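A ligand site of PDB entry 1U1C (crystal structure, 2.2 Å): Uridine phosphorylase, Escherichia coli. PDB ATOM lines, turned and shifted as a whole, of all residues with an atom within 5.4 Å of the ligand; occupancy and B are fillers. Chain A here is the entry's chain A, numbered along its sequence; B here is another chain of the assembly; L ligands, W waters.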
ATOM      1  N   ILE A  72      14.429  29.901 -21.088  1.00  0.00           N
ATOM      2  CA  ILE A  72      14.239  30.838 -19.981  1.00  0.00           C
ATOM      3  C   ILE A  72      14.502  32.258 -20.450  1.00  0.00           C
ATOM      4  O   ILE A  72      15.530  32.536 -21.082  1.00  0.00           O
ATOM      5  CB  ILE A  72      15.181  30.481 -18.793  1.00  0.00           C
ATOM      6  CG1 ILE A  72      14.687  29.227 -18.075  1.00  0.00           C
ATOM      7  CG2 ILE A  72      15.276  31.654 -17.818  1.00  0.00           C
ATOM      8  CD1 ILE A  72      15.792  28.472 -17.366  1.00  0.00           C
ATOM      9  N   THR A  97       6.583  27.034 -14.898  1.00  0.00           N
ATOM     10  CA  THR A  97       6.717  26.789 -13.470  1.00  0.00           C
ATOM     11  C   THR A  97       6.810  28.150 -12.796  1.00  0.00           C
ATOM     12  O   THR A  97       7.216  29.126 -13.427  1.00  0.00           O
ATOM     13  CB  THR A  97       7.976  25.951 -13.172  1.00  0.00           C
ATOM     14  OG1 THR A  97       9.115  26.569 -13.790  1.00  0.00           O
ATOM     15  CG2 THR A  97       7.894  24.578 -13.841  1.00  0.00           C
ATOM     16  N   THR A  98       6.444  28.209 -11.521  1.00  0.00           N
ATOM     17  CA  THR A  98       6.436  29.485 -10.804  1.00  0.00           C
ATOM     18  C   THR A  98       6.581  29.356  -9.278  1.00  0.00           C
ATOM     19  O   THR A  98       6.291  28.311  -8.698  1.00  0.00           O
ATOM     20  CB  THR A  98       5.187  30.313 -11.170  1.00  0.00           C
ATOM     21  OG1 THR A  98       5.255  31.596 -10.548  1.00  0.00           O
ATOM     22  CG2 THR A  98       3.920  29.698 -10.594  1.00  0.00           C
ATOM     23  N   GLY A  99       7.041  30.436  -8.656  1.00  0.00           N
ATOM     24  CA  GLY A  99       7.103  30.533  -7.215  1.00  0.00           C
ATOM     25  C   GLY A  99       6.079  31.534  -6.727  1.00  0.00           C
ATOM     26  O   GLY A  99       6.119  32.703  -7.122  1.00  0.00           O
ATOM     27  N   PHE A 165      16.490  35.285 -12.210  1.00  0.00           N
ATOM     28  CA  PHE A 165      16.004  34.309 -11.237  1.00  0.00           C
ATOM     29  C   PHE A 165      16.368  34.719  -9.802  1.00  0.00           C
ATOM     30  O   PHE A 165      15.585  34.493  -8.876  1.00  0.00           O
ATOM     31  CB  PHE A 165      16.565  32.910 -11.541  1.00  0.00           C
ATOM     32  CG  PHE A 165      15.950  31.813 -10.713  1.00  0.00           C
ATOM     33  CD1 PHE A 165      14.758  31.206 -11.111  1.00  0.00           C
ATOM     34  CD2 PHE A 165      16.559  31.389  -9.534  1.00  0.00           C
ATOM     35  CE1 PHE A 165      14.191  30.181 -10.352  1.00  0.00           C
ATOM     36  CE2 PHE A 165      15.993  30.371  -8.763  1.00  0.00           C
ATOM     37  CZ  PHE A 165      14.800  29.767  -9.171  1.00  0.00           C
ATOM     38  N   GLN A 169      14.178  38.526  -8.122  1.00  0.00           N
ATOM     39  CA  GLN A 169      13.173  37.834  -7.306  1.00  0.00           C
ATOM     40  C   GLN A 169      13.586  37.885  -5.830  1.00  0.00           C
ATOM     41  O   GLN A 169      13.020  37.182  -4.993  1.00  0.00           O
ATOM     42  CB  GLN A 169      12.988  36.387  -7.800  1.00  0.00           C
ATOM     43  CG  GLN A 169      12.556  36.313  -9.269  1.00  0.00           C
ATOM     44  CD  GLN A 169      12.210  34.904  -9.747  1.00  0.00           C
ATOM     45  OE1 GLN A 169      11.730  34.074  -8.974  1.00  0.00           O
ATOM     46  NE2 GLN A 169      12.452  34.647 -11.021  1.00  0.00           N
ATOM     47  N   ARG A 171      16.401  36.973  -4.166  1.00  0.00           N
ATOM     48  CA  ARG A 171      17.111  35.852  -3.549  1.00  0.00           C
ATOM     49  C   ARG A 171      18.474  36.335  -3.058  1.00  0.00           C
ATOM     50  O   ARG A 171      19.246  36.924  -3.838  1.00  0.00           O
ATOM     51  CB  ARG A 171      17.266  34.701  -4.537  1.00  0.00           C
ATOM     52  CG  ARG A 171      15.987  33.914  -4.754  1.00  0.00           C
ATOM     53  CD  ARG A 171      16.146  32.658  -5.606  1.00  0.00           C
ATOM     54  NE  ARG A 171      14.947  31.821  -5.566  1.00  0.00           N
ATOM     55  CZ  ARG A 171      13.909  31.947  -6.376  1.00  0.00           C
ATOM     56  NH1 ARG A 171      13.894  32.870  -7.326  1.00  0.00           N
ATOM     57  NH2 ARG A 171      12.867  31.140  -6.235  1.00  0.00           N
ATOM     58  N   TYR A 198       6.202  34.825  -9.209  1.00  0.00           N
ATOM     59  CA  TYR A 198       7.338  35.157 -10.053  1.00  0.00           C
ATOM     60  C   TYR A 198       7.515  34.100 -11.142  1.00  0.00           C
ATOM     61  O   TYR A 198       7.459  32.894 -10.862  1.00  0.00           O
ATOM     62  CB  TYR A 198       8.634  35.174  -9.241  1.00  0.00           C
ATOM     63  CG  TYR A 198       8.939  36.437  -8.462  1.00  0.00           C
ATOM     64  CD1 TYR A 198       9.069  36.394  -7.077  1.00  0.00           C
ATOM     65  CD2 TYR A 198       9.153  37.659  -9.102  1.00  0.00           C
ATOM     66  CE1 TYR A 198       9.373  37.524  -6.340  1.00  0.00           C
ATOM     67  CE2 TYR A 198       9.465  38.811  -8.370  1.00  0.00           C
ATOM     68  CZ  TYR A 198       9.565  38.729  -6.992  1.00  0.00           C
ATOM     69  OH  TYR A 198       9.870  39.846  -6.249  1.00  0.00           O
ATOM     70  N   GLU A 199       7.737  34.552 -12.373  1.00  0.00           N
ATOM     71  CA  GLU A 199       8.295  33.713 -13.435  1.00  0.00           C
ATOM     72  C   GLU A 199       9.098  34.591 -14.405  1.00  0.00           C
ATOM     73  O   GLU A 199       9.300  35.781 -14.131  1.00  0.00           O
ATOM     74  CB  GLU A 199       7.220  32.839 -14.126  1.00  0.00           C
ATOM     75  CG  GLU A 199       6.017  33.578 -14.676  1.00  0.00           C
ATOM     76  CD  GLU A 199       6.343  34.298 -15.967  1.00  0.00           C
ATOM     77  OE1 GLU A 199       6.403  35.545 -15.938  1.00  0.00           O
ATOM     78  OE2 GLU A 199       6.544  33.633 -17.002  1.00  0.00           O
ATOM     79  N   MET A 200       9.558  34.029 -15.514  1.00  0.00           N
ATOM     80  CA  MET A 200      10.576  34.706 -16.316  1.00  0.00           C
ATOM     81  C   MET A 200      10.311  34.893 -17.825  1.00  0.00           C
ATOM     82  O   MET A 200      11.217  35.311 -18.563  1.00  0.00           O
ATOM     83  CB  MET A 200      11.960  34.054 -16.086  1.00  0.00           C
ATOM     84  CG  MET A 200      12.504  34.233 -14.656  1.00  0.00           C
ATOM     85  SD  MET A 200      14.042  33.362 -14.330  1.00  0.00           S
ATOM     86  CE  MET A 200      15.217  34.339 -15.297  1.00  0.00           C
ATOM     87  N   GLU A 201       9.097  34.610 -18.289  1.00  0.00           N
ATOM     88  CA  GLU A 201       8.794  34.725 -19.730  1.00  0.00           C
ATOM     89  C   GLU A 201       7.517  35.482 -20.103  1.00  0.00           C
ATOM     90  O   GLU A 201       7.388  35.932 -21.246  1.00  0.00           O
ATOM     91  CB  GLU A 201       8.774  33.339 -20.392  1.00  0.00           C
ATOM     92  CG  GLU A 201      10.131  32.689 -20.539  1.00  0.00           C
ATOM     93  CD  GLU A 201      10.402  31.661 -19.461  1.00  0.00           C
ATOM     94  OE1 GLU A 201       9.658  30.656 -19.399  1.00  0.00           O
ATOM     95  OE2 GLU A 201      11.364  31.848 -18.680  1.00  0.00           O
ATOM     96  N   ILE A 223       5.406  25.408  -7.677  1.00  0.00           N
ATOM     97  CA  ILE A 223       6.211  24.339  -7.092  1.00  0.00           C
ATOM     98  C   ILE A 223       6.914  24.813  -5.808  1.00  0.00           C
ATOM     99  O   ILE A 223       7.636  24.042  -5.169  1.00  0.00           O
ATOM    100  CB  ILE A 223       7.230  23.765  -8.114  1.00  0.00           C
ATOM    101  CG1 ILE A 223       8.114  24.868  -8.699  1.00  0.00           C
ATOM    102  CG2 ILE A 223       6.494  22.995  -9.220  1.00  0.00           C
ATOM    103  CD1 ILE A 223       9.429  24.376  -9.288  1.00  0.00           C
ATOM    104  N   VAL A 224       6.670  26.076  -5.449  1.00  0.00           N
ATOM    105  CA  VAL A 224       7.278  26.715  -4.289  1.00  0.00           C
ATOM    106  C   VAL A 224       6.442  27.906  -3.846  1.00  0.00           C
ATOM    107  O   VAL A 224       5.896  28.639  -4.673  1.00  0.00           O
ATOM    108  CB  VAL A 224       8.756  27.146  -4.585  1.00  0.00           C
ATOM    109  CG1 VAL A 224       9.021  28.613  -4.225  1.00  0.00           C
ATOM    110  CG2 VAL A 224       9.736  26.235  -3.873  1.00  0.00           C
ATOM    111  N   ARG A 226       7.194  31.232  -1.565  1.00  0.00           N
ATOM    112  CA  ARG A 226       8.316  31.976  -0.996  1.00  0.00           C
ATOM    113  C   ARG A 226       8.164  32.313   0.490  1.00  0.00           C
ATOM    114  O   ARG A 226       9.153  32.506   1.185  1.00  0.00           O
ATOM    115  CB  ARG A 226       8.612  33.232  -1.819  1.00  0.00           C
ATOM    116  CG  ARG A 226       9.127  32.971  -3.224  1.00  0.00           C
ATOM    117  CD  ARG A 226      10.571  32.455  -3.301  1.00  0.00           C
ATOM    118  NE  ARG A 226      11.555  33.408  -2.793  1.00  0.00           N
ATOM    119  CZ  ARG A 226      12.062  34.431  -3.479  1.00  0.00           C
ATOM    120  NH1 ARG A 226      11.682  34.657  -4.735  1.00  0.00           N
ATOM    121  NH2 ARG A 226      12.950  35.229  -2.908  1.00  0.00           N
ATOM    122  N   GLU A 230      11.949  27.616   0.109  1.00  0.00           N
ATOM    123  CA  GLU A 230      12.787  28.055  -1.003  1.00  0.00           C
ATOM    124  C   GLU A 230      13.095  26.911  -1.982  1.00  0.00           C
ATOM    125  O   GLU A 230      13.086  27.110  -3.201  1.00  0.00           O
ATOM    126  CB  GLU A 230      14.089  28.685  -0.478  1.00  0.00           C
ATOM    127  CG  GLU A 230      15.188  28.930  -1.513  1.00  0.00           C
ATOM    128  CD  GLU A 230      14.830  29.971  -2.562  1.00  0.00           C
ATOM    129  OE1 GLU A 230      15.588  30.090  -3.549  1.00  0.00           O
ATOM    130  OE2 GLU A 230      13.805  30.681  -2.418  1.00  0.00           O
ATOM    131  N   ILE A 231      13.349  25.718  -1.452  1.00  0.00           N
ATOM    132  CA  ILE A 231      13.641  24.546  -2.277  1.00  0.00           C
ATOM    133  C   ILE A 231      12.362  23.757  -2.559  1.00  0.00           C
ATOM    134  O   ILE A 231      11.646  23.382  -1.627  1.00  0.00           O
ATOM    135  CB  ILE A 231      14.734  23.650  -1.621  1.00  0.00           C
ATOM    136  CG1 ILE A 231      16.039  24.438  -1.439  1.00  0.00           C
ATOM    137  CG2 ILE A 231      14.978  22.385  -2.447  1.00  0.00           C
ATOM    138  CD1 ILE A 231      16.993  23.851  -0.421  1.00  0.00           C
ATOM    139  N   PRO A 232      12.076  23.508  -3.841  1.00  0.00           N
ATOM    140  CA  PRO A 232      10.891  22.741  -4.227  1.00  0.00           C
ATOM    141  C   PRO A 232      11.057  21.242  -3.957  1.00  0.00           C
ATOM    142  O   PRO A 232      12.165  20.724  -3.980  1.00  0.00           O
ATOM    143  CB  PRO A 232      10.784  22.991  -5.742  1.00  0.00           C
ATOM    144  CG  PRO A 232      12.186  23.288  -6.174  1.00  0.00           C
ATOM    145  CD  PRO A 232      12.854  23.958  -5.014  1.00  0.00           C
ATOM    146  N   PHE B  10      20.552  25.024  -8.529  1.00  0.00           N
ATOM    147  CA  PHE B  10      19.141  24.890  -8.925  1.00  0.00           C
ATOM    148  C   PHE B  10      18.910  24.406 -10.363  1.00  0.00           C
ATOM    149  O   PHE B  10      17.958  23.666 -10.609  1.00  0.00           O
ATOM    150  CB  PHE B  10      18.407  26.224  -8.708  1.00  0.00           C
ATOM    151  CG  PHE B  10      17.914  26.442  -7.299  1.00  0.00           C
ATOM    152  CD1 PHE B  10      17.858  27.721  -6.764  1.00  0.00           C
ATOM    153  CD2 PHE B  10      17.506  25.373  -6.506  1.00  0.00           C
ATOM    154  CE1 PHE B  10      17.409  27.942  -5.467  1.00  0.00           C
ATOM    155  CE2 PHE B  10      17.058  25.572  -5.205  1.00  0.00           C
ATOM    156  CZ  PHE B  10      17.009  26.868  -4.688  1.00  0.00           C
ATOM    157  N   HIS B  11      19.756  24.821 -11.293  1.00  0.00           N
ATOM    158  CA  HIS B  11      19.509  24.574 -12.718  1.00  0.00           C
ATOM    159  C   HIS B  11      20.543  23.721 -13.449  1.00  0.00           C
ATOM    160  O   HIS B  11      20.186  22.879 -14.268  1.00  0.00           O
ATOM    161  CB  HIS B  11      19.317  25.899 -13.473  1.00  0.00           C
ATOM    162  CG  HIS B  11      18.149  26.691 -12.983  1.00  0.00           C
ATOM    163  ND1 HIS B  11      18.241  27.596 -11.953  1.00  0.00           N
ATOM    164  CD2 HIS B  11      16.861  26.717 -13.391  1.00  0.00           C
ATOM    165  CE1 HIS B  11      17.060  28.140 -11.740  1.00  0.00           C
ATOM    166  NE2 HIS B  11      16.200  27.630 -12.597  1.00  0.00           N
ATOM    167  N   ARG B  51      17.750  21.782 -19.460  1.00  0.00           N
ATOM    168  CA  ARG B  51      17.187  22.937 -20.164  1.00  0.00           C
ATOM    169  C   ARG B  51      18.147  23.376 -21.275  1.00  0.00           C
ATOM    170  O   ARG B  51      18.558  22.557 -22.095  1.00  0.00           O
ATOM    171  CB  ARG B  51      16.899  24.093 -19.185  1.00  0.00           C
ATOM    172  CG  ARG B  51      15.773  23.839 -18.191  1.00  0.00           C
ATOM    173  CD  ARG B  51      15.588  24.979 -17.202  1.00  0.00           C
ATOM    174  NE  ARG B  51      14.366  24.874 -16.411  1.00  0.00           N
ATOM    175  CZ  ARG B  51      13.220  25.492 -16.679  1.00  0.00           C
ATOM    176  NH1 ARG B  51      13.111  26.267 -17.755  1.00  0.00           N
ATOM    177  NH2 ARG B  51      12.171  25.324 -15.893  1.00  0.00           N
ATOM    178  N   ILE B  79      21.491  33.157 -14.777  1.00  0.00           N
ATOM    179  CA  ILE B  79      21.365  31.902 -14.034  1.00  0.00           C
ATOM    180  C   ILE B  79      22.658  31.074 -14.110  1.00  0.00           C
ATOM    181  O   ILE B  79      23.184  30.635 -13.081  1.00  0.00           O
ATOM    182  CB  ILE B  79      20.157  31.052 -14.526  1.00  0.00           C
ATOM    183  CG1 ILE B  79      18.833  31.736 -14.152  1.00  0.00           C
ATOM    184  CG2 ILE B  79      20.211  29.634 -13.970  1.00  0.00           C
ATOM    185  CD1 ILE B  79      17.610  31.129 -14.820  1.00  0.00           C
HETATM  186  O1  LIG L   1      13.647  27.834 -13.168  1.00  0.00           O
HETATM  187  C1  LIG L   1      13.437  28.794 -14.128  1.00  0.00           C
HETATM  188  C2  LIG L   1      12.189  29.582 -14.231  1.00  0.00           C
HETATM  189  O2  LIG L   1      10.985  29.069 -13.951  1.00  0.00           O
HETATM  190  C3  LIG L   1      10.370  30.017 -13.238  1.00  0.00           C
HETATM  191  N1  LIG L   1      10.491  30.264 -11.909  1.00  0.00           N
HETATM  192  C4  LIG L   1      10.808  31.583 -11.380  1.00  0.00           C
HETATM  193  O3  LIG L   1      11.040  32.583 -12.081  1.00  0.00           O
HETATM  194  N2  LIG L   1      10.907  31.698  -9.961  1.00  0.00           N
HETATM  195  C5  LIG L   1      10.703  30.585  -9.098  1.00  0.00           C
HETATM  196  O4  LIG L   1      10.821  30.779  -7.870  1.00  0.00           O
HETATM  197  C6  LIG L   1      10.292  29.152 -11.015  1.00  0.00           C
HETATM  198  C7  LIG L   1      10.398  29.273  -9.616  1.00  0.00           C
HETATM  199  C8  LIG L   1      10.290  27.993  -8.694  1.00  0.00           C
HETATM  200  C9  LIG L   1      11.656  27.446  -8.291  1.00  0.00           C
HETATM  201  C10 LIG L   1      12.445  26.656  -9.216  1.00  0.00           C
HETATM  202  C11 LIG L   1      13.761  26.203  -8.850  1.00  0.00           C
HETATM  203  C12 LIG L   1      14.280  26.538  -7.548  1.00  0.00           C
HETATM  204  C13 LIG L   1      13.500  27.321  -6.637  1.00  0.00           C
HETATM  205  C14 LIG L   1      12.185  27.780  -6.990  1.00  0.00           C
HETATM  206  O   HOH W   1      11.490  26.380 -12.655  1.00  0.00           O
HETATM  207  O   HOH W   2      10.219  33.332  -6.829  1.00  0.00           O
HETATM  208  O   HOH W   3      10.117  31.238 -16.293  1.00  0.00           O
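Water W1 lies within hydrogen-bond range of OG1 of Thr 97, O1 of the ligand and NH2 of Arg 51 of chain B.
Water W2 lies within hydrogen-bond range of OE1 of Gln 169 (2.7 Å), O4 of the ligand (2.8 Å), NH1 of Arg 226 (2.9 Å) and NH2 of Arg 171 (3.5 Å).
Water W3 lies within hydrogen-bond range of the side-chain carboxylate of Glu 201 (2.8 Å), the backbone NH of Met 200 (3.0 Å) and an oxygen (O2) of the ligand (3.3 Å).
An oxygen (O4) of the ligand is in hydrogen-bond range of the guanidinium group of Arg 171, at 2.6 Å.
A ring nitrogen (NE2) of His 11 of chain B lies within hydrogen-bond range of an oxygen (O1) of the ligand (2.6 Å).
OG1 of Thr 97 lies within hydrogen-bond range of O2 of the ligand, 3.1 Å away.
OE1 of Gln 169 sits at hydrogen-bond distance from N2 of the ligand (2.7 Å).
Residues that only touch the ligand: Thr 98, Gly 99, Phe 165, Tyr 198, Glu 199, Met 200, Ile 223, Glu 230, Pro 232, Phe 10 of chain B and Arg 51 of chain B.
Hydrophobic or aromatic side chains within 4 Å of the ligand: Phe 165, Met 200, Ile 223, Pro 232, Phe 10 of chain B and His 11 of chain B.
The nearest printed residue that does not touch the ligand is Ile 72 (4.02 Å).
The guanidinium group of Arg 171 lies within hydrogen-bond range of the backbone carbonyl oxygen of Phe 165.
The backbone carbonyl oxygen of Tyr 198 is in hydrogen-bond range of the side-chain hydroxyl of Thr 98 (2.6 Å).
The backbone NH (N) of Phe 165 lies close to the side-chain sulfur (SD) of Met 200 (3.8 Å).
NE of Arg 226 lies within salt-bridge range of OE2 of Glu 230 (3.6 Å).
N of Ile 223 sits at hydrogen-bond distance from O of Thr 98, at 3.2 Å.
NH2 of Arg 226 sits at hydrogen-bond distance from O of Gln 169 (2.9 Å).
OE1 of Glu 230 is in salt-bridge range of NE of Arg 171, at 2.7 Å.
The guanidinium group (NH1) of Arg 171 sits at hydrogen-bond distance from the side-chain amide oxygen (OE1) of Gln 169.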
